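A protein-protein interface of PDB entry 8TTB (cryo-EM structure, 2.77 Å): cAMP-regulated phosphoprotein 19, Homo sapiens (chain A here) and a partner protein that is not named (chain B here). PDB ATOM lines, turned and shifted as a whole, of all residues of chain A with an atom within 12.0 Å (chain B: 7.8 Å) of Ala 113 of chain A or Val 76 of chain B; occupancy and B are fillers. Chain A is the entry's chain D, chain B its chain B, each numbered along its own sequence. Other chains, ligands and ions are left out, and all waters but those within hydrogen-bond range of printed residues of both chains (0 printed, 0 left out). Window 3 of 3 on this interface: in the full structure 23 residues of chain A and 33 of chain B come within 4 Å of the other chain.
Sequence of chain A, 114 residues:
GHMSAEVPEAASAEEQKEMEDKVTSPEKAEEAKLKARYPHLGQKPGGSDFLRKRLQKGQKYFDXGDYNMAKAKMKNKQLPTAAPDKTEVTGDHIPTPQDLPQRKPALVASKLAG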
ATOM      1  N   LEU A 107      25.783 -37.433  12.679  1.00  0.00           N
ATOM      2  CA  LEU A 107      25.302 -36.367  13.547  1.00  0.00           C
ATOM      3  C   LEU A 107      24.873 -35.175  12.703  1.00  0.00           C
ATOM      4  O   LEU A 107      25.584 -34.776  11.775  1.00  0.00           O
ATOM      5  CB  LEU A 107      26.382 -35.947  14.546  1.00  0.00           C
ATOM      6  CG  LEU A 107      25.958 -34.930  15.609  1.00  0.00           C
ATOM      7  CD1 LEU A 107      24.816 -35.473  16.454  1.00  0.00           C
ATOM      8  CD2 LEU A 107      27.140 -34.556  16.486  1.00  0.00           C
ATOM      9  N   VAL A 108      23.709 -34.614  13.028  1.00  0.00           N
ATOM     10  CA  VAL A 108      23.152 -33.483  12.294  1.00  0.00           C
ATOM     11  C   VAL A 108      23.786 -32.189  12.784  1.00  0.00           C
ATOM     12  O   VAL A 108      24.479 -32.170  13.807  1.00  0.00           O
ATOM     13  CB  VAL A 108      21.620 -33.429  12.435  1.00  0.00           C
ATOM     14  CG1 VAL A 108      20.993 -34.698  11.878  1.00  0.00           C
ATOM     15  CG2 VAL A 108      21.221 -33.222  13.890  1.00  0.00           C
ATOM     16  N   ALA A 109      23.553 -31.102  12.055  1.00  0.00           N
ATOM     17  CA  ALA A 109      24.115 -29.814  12.430  1.00  0.00           C
ATOM     18  C   ALA A 109      23.546 -29.346  13.765  1.00  0.00           C
ATOM     19  O   ALA A 109      22.406 -29.650  14.123  1.00  0.00           O
ATOM     20  CB  ALA A 109      23.829 -28.772  11.348  1.00  0.00           C
ATOM     21  N   SER A 110      24.360 -28.595  14.501  1.00  0.00           N
ATOM     22  CA  SER A 110      23.955 -28.116  15.813  1.00  0.00           C
ATOM     23  C   SER A 110      22.742 -27.201  15.701  1.00  0.00           C
ATOM     24  O   SER A 110      22.589 -26.446  14.739  1.00  0.00           O
ATOM     25  CB  SER A 110      25.108 -27.371  16.484  1.00  0.00           C
ATOM     26  OG  SER A 110      24.712 -26.849  17.739  1.00  0.00           O
ATOM     27  N   LYS A 111      21.869 -27.280  16.706  1.00  0.00           N
ATOM     28  CA  LYS A 111      20.689 -26.426  16.735  1.00  0.00           C
ATOM     29  C   LYS A 111      21.046 -24.959  16.917  1.00  0.00           C
ATOM     30  O   LYS A 111      20.234 -24.091  16.581  1.00  0.00           O
ATOM     31  CB  LYS A 111      19.747 -26.880  17.848  1.00  0.00           C
ATOM     32  CG  LYS A 111      19.224 -28.294  17.661  1.00  0.00           C
ATOM     33  CD  LYS A 111      18.416 -28.758  18.857  1.00  0.00           C
ATOM     34  CE  LYS A 111      17.913 -30.178  18.667  1.00  0.00           C
ATOM     35  NZ  LYS A 111      17.196 -30.685  19.869  1.00  0.00           N
ATOM     36  N   LEU A 112      22.236 -24.660  17.442  1.00  0.00           N
ATOM     37  CA  LEU A 112      22.675 -23.272  17.522  1.00  0.00           C
ATOM     38  C   LEU A 112      22.807 -22.664  16.133  1.00  0.00           C
ATOM     39  O   LEU A 112      22.429 -21.509  15.912  1.00  0.00           O
ATOM     40  CB  LEU A 112      24.004 -23.184  18.270  1.00  0.00           C
ATOM     41  CG  LEU A 112      23.979 -23.530  19.757  1.00  0.00           C
ATOM     42  CD1 LEU A 112      25.392 -23.595  20.303  1.00  0.00           C
ATOM     43  CD2 LEU A 112      23.160 -22.518  20.531  1.00  0.00           C
ATOM     44  N   ALA A 113      23.344 -23.430  15.181  1.00  0.00           N
ATOM     45  CA  ALA A 113      23.491 -22.933  13.820  1.00  0.00           C
ATOM     46  C   ALA A 113      22.150 -22.659  13.159  1.00  0.00           C
ATOM     47  O   ALA A 113      22.096 -21.912  12.178  1.00  0.00           O
ATOM     48  CB  ALA A 113      24.286 -23.934  12.982  1.00  0.00           C
ATOM     49  N   GLY A 114      21.070 -23.243  13.668  1.00  0.00           N
ATOM     50  CA  GLY A 114      19.751 -23.034  13.102  1.00  0.00           C
ATOM     51  C   GLY A 114      19.335 -21.576  13.112  1.00  0.00           C
ATOM     52  O   GLY A 114      20.003 -20.731  13.707  1.00  0.00           O
ATOM     53  OXT GLY A 114      18.321 -21.201  12.525  1.00  0.00           O
ATOM     54  N   GLN B  19      20.620 -11.404  22.424  1.00  0.00           N
ATOM     55  CA  GLN B  19      20.303 -12.544  21.580  1.00  0.00           C
ATOM     56  C   GLN B  19      20.228 -13.800  22.430  1.00  0.00           C
ATOM     57  O   GLN B  19      20.796 -13.874  23.522  1.00  0.00           O
ATOM     58  CB  GLN B  19      21.343 -12.742  20.474  1.00  0.00           C
ATOM     59  CG  GLN B  19      21.541 -11.546  19.574  1.00  0.00           C
ATOM     60  CD  GLN B  19      22.518 -11.832  18.459  1.00  0.00           C
ATOM     61  OE1 GLN B  19      23.594 -11.241  18.396  1.00  0.00           O
ATOM     62  NE2 GLN B  19      22.151 -12.746  17.570  1.00  0.00           N
ATOM     63  N   LYS B  21      20.334 -18.149  21.403  1.00  0.00           N
ATOM     64  CA  LYS B  21      20.513 -19.105  20.324  1.00  0.00           C
ATOM     65  C   LYS B  21      20.317 -20.518  20.850  1.00  0.00           C
ATOM     66  O   LYS B  21      20.600 -20.812  22.013  1.00  0.00           O
ATOM     67  CB  LYS B  21      21.893 -18.956  19.686  1.00  0.00           C
ATOM     68  CG  LYS B  21      22.128 -17.569  19.123  1.00  0.00           C
ATOM     69  CD  LYS B  21      23.331 -17.526  18.207  1.00  0.00           C
ATOM     70  CE  LYS B  21      23.462 -16.169  17.537  1.00  0.00           C
ATOM     71  NZ  LYS B  21      22.293 -15.854  16.673  1.00  0.00           N
ATOM     72  N   GLY B  22      19.822 -21.383  19.978  1.00  0.00           N
ATOM     73  CA  GLY B  22      19.470 -22.742  20.333  1.00  0.00           C
ATOM     74  C   GLY B  22      17.965 -22.936  20.393  1.00  0.00           C
ATOM     75  O   GLY B  22      17.177 -21.989  20.402  1.00  0.00           O
ATOM     76  N   LEU B  45      34.666 -12.893  16.356  1.00  0.00           N
ATOM     77  CA  LEU B  45      34.172 -14.258  16.286  1.00  0.00           C
ATOM     78  C   LEU B  45      33.967 -14.825  17.684  1.00  0.00           C
ATOM     79  O   LEU B  45      34.688 -14.480  18.625  1.00  0.00           O
ATOM     80  CB  LEU B  45      35.138 -15.148  15.501  1.00  0.00           C
ATOM     81  CG  LEU B  45      35.405 -14.717  14.060  1.00  0.00           C
ATOM     82  CD1 LEU B  45      36.419 -15.639  13.418  1.00  0.00           C
ATOM     83  CD2 LEU B  45      34.120 -14.698  13.253  1.00  0.00           C
ATOM     84  N   VAL B  55      31.276 -27.649  16.664  1.00  0.00           N
ATOM     85  CA  VAL B  55      31.744 -26.298  16.939  1.00  0.00           C
ATOM     86  C   VAL B  55      30.975 -25.340  16.044  1.00  0.00           C
ATOM     87  O   VAL B  55      30.925 -25.529  14.825  1.00  0.00           O
ATOM     88  CB  VAL B  55      33.259 -26.163  16.711  1.00  0.00           C
ATOM     89  CG1 VAL B  55      33.675 -24.703  16.762  1.00  0.00           C
ATOM     90  CG2 VAL B  55      34.018 -26.968  17.747  1.00  0.00           C
ATOM     91  N   VAL B  56      30.376 -24.321  16.650  1.00  0.00           N
ATOM     92  CA  VAL B  56      29.630 -23.295  15.936  1.00  0.00           C
ATOM     93  C   VAL B  56      30.299 -21.957  16.208  1.00  0.00           C
ATOM     94  O   VAL B  56      30.486 -21.577  17.368  1.00  0.00           O
ATOM     95  CB  VAL B  56      28.152 -23.263  16.363  1.00  0.00           C
ATOM     96  CG1 VAL B  56      27.398 -22.205  15.582  1.00  0.00           C
ATOM     97  CG2 VAL B  56      27.518 -24.626  16.168  1.00  0.00           C
ATOM     98  N   ILE B  57      30.651 -21.245  15.141  1.00  0.00           N
ATOM     99  CA  ILE B  57      31.341 -19.966  15.231  1.00  0.00           C
ATOM    100  C   ILE B  57      30.382 -18.874  14.784  1.00  0.00           C
ATOM    101  O   ILE B  57      29.802 -18.956  13.696  1.00  0.00           O
ATOM    102  CB  ILE B  57      32.622 -19.958  14.381  1.00  0.00           C
ATOM    103  CG1 ILE B  57      33.564 -21.070  14.846  1.00  0.00           C
ATOM    104  CG2 ILE B  57      33.308 -18.603  14.468  1.00  0.00           C
ATOM    105  CD1 ILE B  57      34.805 -21.216  14.006  1.00  0.00           C
ATOM    106  N   PHE B  58      30.215 -17.858  15.624  1.00  0.00           N
ATOM    107  CA  PHE B  58      29.358 -16.720  15.333  1.00  0.00           C
ATOM    108  C   PHE B  58      30.216 -15.489  15.084  1.00  0.00           C
ATOM    109  O   PHE B  58      31.197 -15.254  15.793  1.00  0.00           O
ATOM    110  CB  PHE B  58      28.394 -16.447  16.487  1.00  0.00           C
ATOM    111  CG  PHE B  58      27.622 -17.653  16.925  1.00  0.00           C
ATOM    112  CD1 PHE B  58      26.431 -17.988  16.311  1.00  0.00           C
ATOM    113  CD2 PHE B  58      28.086 -18.449  17.954  1.00  0.00           C
ATOM    114  CE1 PHE B  58      25.722 -19.095  16.713  1.00  0.00           C
ATOM    115  CE2 PHE B  58      27.379 -19.557  18.360  1.00  0.00           C
ATOM    116  CZ  PHE B  58      26.195 -19.880  17.739  1.00  0.00           C
ATOM    117  N   GLN B  59      29.839 -14.705  14.079  1.00  0.00           N
ATOM    118  CA  GLN B  59      30.560 -13.495  13.710  1.00  0.00           C
ATOM    119  C   GLN B  59      29.676 -12.283  13.961  1.00  0.00           C
ATOM    120  O   GLN B  59      28.498 -12.279  13.589  1.00  0.00           O
ATOM    121  CB  GLN B  59      30.990 -13.538  12.243  1.00  0.00           C
ATOM    122  CG  GLN B  59      31.816 -12.342  11.809  1.00  0.00           C
ATOM    123  CD  GLN B  59      32.221 -12.416  10.355  1.00  0.00           C
ATOM    124  OE1 GLN B  59      31.447 -12.851   9.505  1.00  0.00           O
ATOM    125  NE2 GLN B  59      33.445 -11.996  10.060  1.00  0.00           N
ATOM    126  N   GLN B  60      30.244 -11.262  14.593  1.00  0.00           N
ATOM    127  CA  GLN B  60      29.504 -10.038  14.854  1.00  0.00           C
ATOM    128  C   GLN B  60      29.318  -9.246  13.566  1.00  0.00           C
ATOM    129  O   GLN B  60      30.207  -9.201  12.712  1.00  0.00           O
ATOM    130  CB  GLN B  60      30.238  -9.189  15.888  1.00  0.00           C
ATOM    131  CG  GLN B  60      29.443  -8.005  16.392  1.00  0.00           C
ATOM    132  CD  GLN B  60      30.195  -7.202  17.429  1.00  0.00           C
ATOM    133  OE1 GLN B  60      31.423  -7.238  17.485  1.00  0.00           O
ATOM    134  NE2 GLN B  60      29.462  -6.473  18.259  1.00  0.00           N
ATOM    135  N   GLU B  73      24.718  -7.628  16.232  1.00  0.00           N
ATOM    136  CA  GLU B  73      24.346  -8.975  16.624  1.00  0.00           C
ATOM    137  C   GLU B  73      25.333  -9.991  16.059  1.00  0.00           C
ATOM    138  O   GLU B  73      26.023  -9.745  15.067  1.00  0.00           O
ATOM    139  CB  GLU B  73      22.930  -9.298  16.148  1.00  0.00           C
ATOM    140  CG  GLU B  73      21.844  -8.533  16.883  1.00  0.00           C
ATOM    141  CD  GLU B  73      20.451  -8.970  16.478  1.00  0.00           C
ATOM    142  OE1 GLU B  73      20.336  -9.831  15.581  1.00  0.00           O
ATOM    143  OE2 GLU B  73      19.473  -8.455  17.057  1.00  0.00           O
ATOM    144  N   TYR B  74      25.395 -11.146  16.712  1.00  0.00           N
ATOM    145  CA  TYR B  74      26.248 -12.245  16.286  1.00  0.00           C
ATOM    146  C   TYR B  74      25.438 -13.211  15.434  1.00  0.00           C
ATOM    147  O   TYR B  74      24.363 -13.657  15.846  1.00  0.00           O
ATOM    148  CB  TYR B  74      26.843 -12.972  17.491  1.00  0.00           C
ATOM    149  CG  TYR B  74      28.016 -12.255  18.110  1.00  0.00           C
ATOM    150  CD1 TYR B  74      27.823 -11.197  18.985  1.00  0.00           C
ATOM    151  CD2 TYR B  74      29.317 -12.633  17.818  1.00  0.00           C
ATOM    152  CE1 TYR B  74      28.893 -10.539  19.551  1.00  0.00           C
ATOM    153  CE2 TYR B  74      30.390 -11.982  18.379  1.00  0.00           C
ATOM    154  CZ  TYR B  74      30.173 -10.935  19.245  1.00  0.00           C
ATOM    155  OH  TYR B  74      31.243 -10.281  19.806  1.00  0.00           O
ATOM    156  N   ASN B  75      25.958 -13.532  14.254  1.00  0.00           N
ATOM    157  CA  ASN B  75      25.292 -14.414  13.311  1.00  0.00           C
ATOM    158  C   ASN B  75      26.180 -15.613  13.015  1.00  0.00           C
ATOM    159  O   ASN B  75      27.407 -15.538  13.117  1.00  0.00           O
ATOM    160  CB  ASN B  75      24.959 -13.682  12.007  1.00  0.00           C
ATOM    161  CG  ASN B  75      24.032 -12.508  12.222  1.00  0.00           C
ATOM    162  OD1 ASN B  75      23.119 -12.565  13.045  1.00  0.00           O
ATOM    163  ND2 ASN B  75      24.264 -11.430  11.485  1.00  0.00           N
ATOM    164  N   VAL B  76      25.543 -16.724  12.644  1.00  0.00           N
ATOM    165  CA  VAL B  76      26.282 -17.948  12.371  1.00  0.00           C
ATOM    166  C   VAL B  76      27.312 -17.681  11.288  1.00  0.00           C
ATOM    167  O   VAL B  76      27.005 -17.099  10.241  1.00  0.00           O
ATOM    168  CB  VAL B  76      25.321 -19.072  11.962  1.00  0.00           C
ATOM    169  CG1 VAL B  76      26.071 -20.388  11.838  1.00  0.00           C
ATOM    170  CG2 VAL B  76      24.186 -19.186  12.962  1.00  0.00           C
ATOM    171  N   TYR B  77      28.547 -18.109  11.538  1.00  0.00           N
ATOM    172  CA  TYR B  77      29.659 -17.906  10.619  1.00  0.00           C
ATOM    173  C   TYR B  77      30.202 -19.214  10.071  1.00  0.00           C
ATOM    174  O   TYR B  77      30.346 -19.363   8.854  1.00  0.00           O
ATOM    175  CB  TYR B  77      30.774 -17.129  11.331  1.00  0.00           C
ATOM    176  CG  TYR B  77      31.990 -16.858  10.481  1.00  0.00           C
ATOM    177  CD1 TYR B  77      31.972 -15.879   9.499  1.00  0.00           C
ATOM    178  CD2 TYR B  77      33.166 -17.567  10.673  1.00  0.00           C
ATOM    179  CE1 TYR B  77      33.084 -15.625   8.726  1.00  0.00           C
ATOM    180  CE2 TYR B  77      34.282 -17.319   9.907  1.00  0.00           C
ATOM    181  CZ  TYR B  77      34.236 -16.347   8.934  1.00  0.00           C
ATOM    182  OH  TYR B  77      35.349 -16.097   8.170  1.00  0.00           O
ATOM    183  N   SER B  78      30.502 -20.175  10.940  1.00  0.00           N
ATOM    184  CA  SER B  78      31.006 -21.469  10.509  1.00  0.00           C
ATOM    185  C   SER B  78      30.467 -22.542  11.441  1.00  0.00           C
ATOM    186  O   SER B  78      30.098 -22.271  12.586  1.00  0.00           O
ATOM    187  CB  SER B  78      32.537 -21.498  10.488  1.00  0.00           C
ATOM    188  OG  SER B  78      33.014 -22.754  10.041  1.00  0.00           O
ATOM    189  N   THR B  79      30.426 -23.768  10.931  1.00  0.00           N
ATOM    190  CA  THR B  79      29.970 -24.914  11.706  1.00  0.00           C
ATOM    191  C   THR B  79      30.676 -26.152  11.183  1.00  0.00           C
ATOM    192  O   THR B  79      30.728 -26.368   9.969  1.00  0.00           O
ATOM    193  CB  THR B  79      28.451 -25.086  11.606  1.00  0.00           C
ATOM    194  OG1 THR B  79      27.799 -23.873  12.003  1.00  0.00           O
ATOM    195  CG2 THR B  79      27.982 -26.225  12.498  1.00  0.00           C
ATOM    196  N   PHE B  80      31.215 -26.958  12.091  1.00  0.00           N
ATOM    197  CA  PHE B  80      31.939 -28.155  11.687  1.00  0.00           C
ATOM    198  C   PHE B  80      31.959 -29.140  12.843  1.00  0.00           C
ATOM    199  O   PHE B  80      31.736 -28.778  14.000  1.00  0.00           O
ATOM    200  CB  PHE B  80      33.363 -27.817  11.235  1.00  0.00           C
ATOM    201  CG  PHE B  80      34.145 -27.020  12.238  1.00  0.00           C
ATOM    202  CD1 PHE B  80      34.006 -25.646  12.307  1.00  0.00           C
ATOM    203  CD2 PHE B  80      35.022 -27.643  13.104  1.00  0.00           C
ATOM    204  CE1 PHE B  80      34.724 -24.911  13.225  1.00  0.00           C
ATOM    205  CE2 PHE B  80      35.743 -26.912  14.024  1.00  0.00           C
ATOM    206  CZ  PHE B  80      35.593 -25.544  14.084  1.00  0.00           C
ATOM    207  N   VAL B 167      32.313 -20.046   3.983  1.00  0.00           N
ATOM    208  CA  VAL B 167      33.285 -20.233   5.052  1.00  0.00           C
ATOM    209  C   VAL B 167      33.594 -21.718   5.160  1.00  0.00           C
ATOM    210  O   VAL B 167      32.680 -22.544   5.274  1.00  0.00           O
ATOM    211  CB  VAL B 167      32.759 -19.680   6.386  1.00  0.00           C
ATOM    212  CG1 VAL B 167      33.815 -19.811   7.467  1.00  0.00           C
ATOM    213  CG2 VAL B 167      32.328 -18.232   6.226  1.00  0.00           C
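O of Tyr 74 of chain B lies within hydrogen-bond range of NZ of Lys 21 of chain B, 3.1 Å away. NE2 of Gln 19 of chain B sits close to NZ of Lys 21 of chain B. The backbone NH (N) of Leu 112 of chain A lies close to the side-chain hydroxyl (OG) of Ser 110 of chain A, 3.3 Å away.
Val 56 of chain B touches Ser 110 of chain A (CG2 to CB, 3.7 Å). O of Lys 21 of chain B touches CD2 of Leu 112 of chain A (3.4 Å). Gly 22 of chain B touches Leu 112 of chain A (N to CD2, 3.6 Å). Leu 112 of chain A touches Phe 58 of chain B. Val 76 of chain B touches Ala 113 of chain A (CG2 to O, 3.5 Å). Ala 113 of chain A touches Thr 79 of chain B.
Of the printed residues of chain B, Leu 112 of chain A touches Lys 21, Gly 22 and Phe 58. Ala 113 of chain A touches just these residues of chain B: Val 76 (3.5 Å) and Thr 79 (3.6 Å). Of the printed residues of chain A, Lys 21 of chain B touches Leu 112. Of chain A, only Ala 113 (3.5 Å) comes within 4 Å of Val 76 of chain B. Thr 79 of chain B touches one residue of chain A. The nearest residue of chain B that does not touch Ala 113 of chain A is Val 56 of chain B (4.3 Å). The nearest printed residue of chain B that does not touch Leu 112 of chain A is Val 76 of chain B (4.1 Å).
Of the 8 printed residues of chain A, 3 touch a printed residue of chain B. Printed residues of chain A that touch a printed residue of chain B: Ser 110, Leu 112 and Ala 113. Of the 19 printed residues of chain B, 6 touch a printed residue of chain A. Printed residues of chain B that touch a printed residue of chain A: Lys 21, Gly 22, Val 56, Phe 58, Val 76 and Thr 79. Hydrophobic or aromatic side chains of chain B within 4 Å of the printed part of chain A: Val 56, Phe 58 and Val 76. Among the printed residues, no Asp or Glu carboxylate lies within 4 Å of a Lys or Arg side-chain nitrogen of the other chain.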
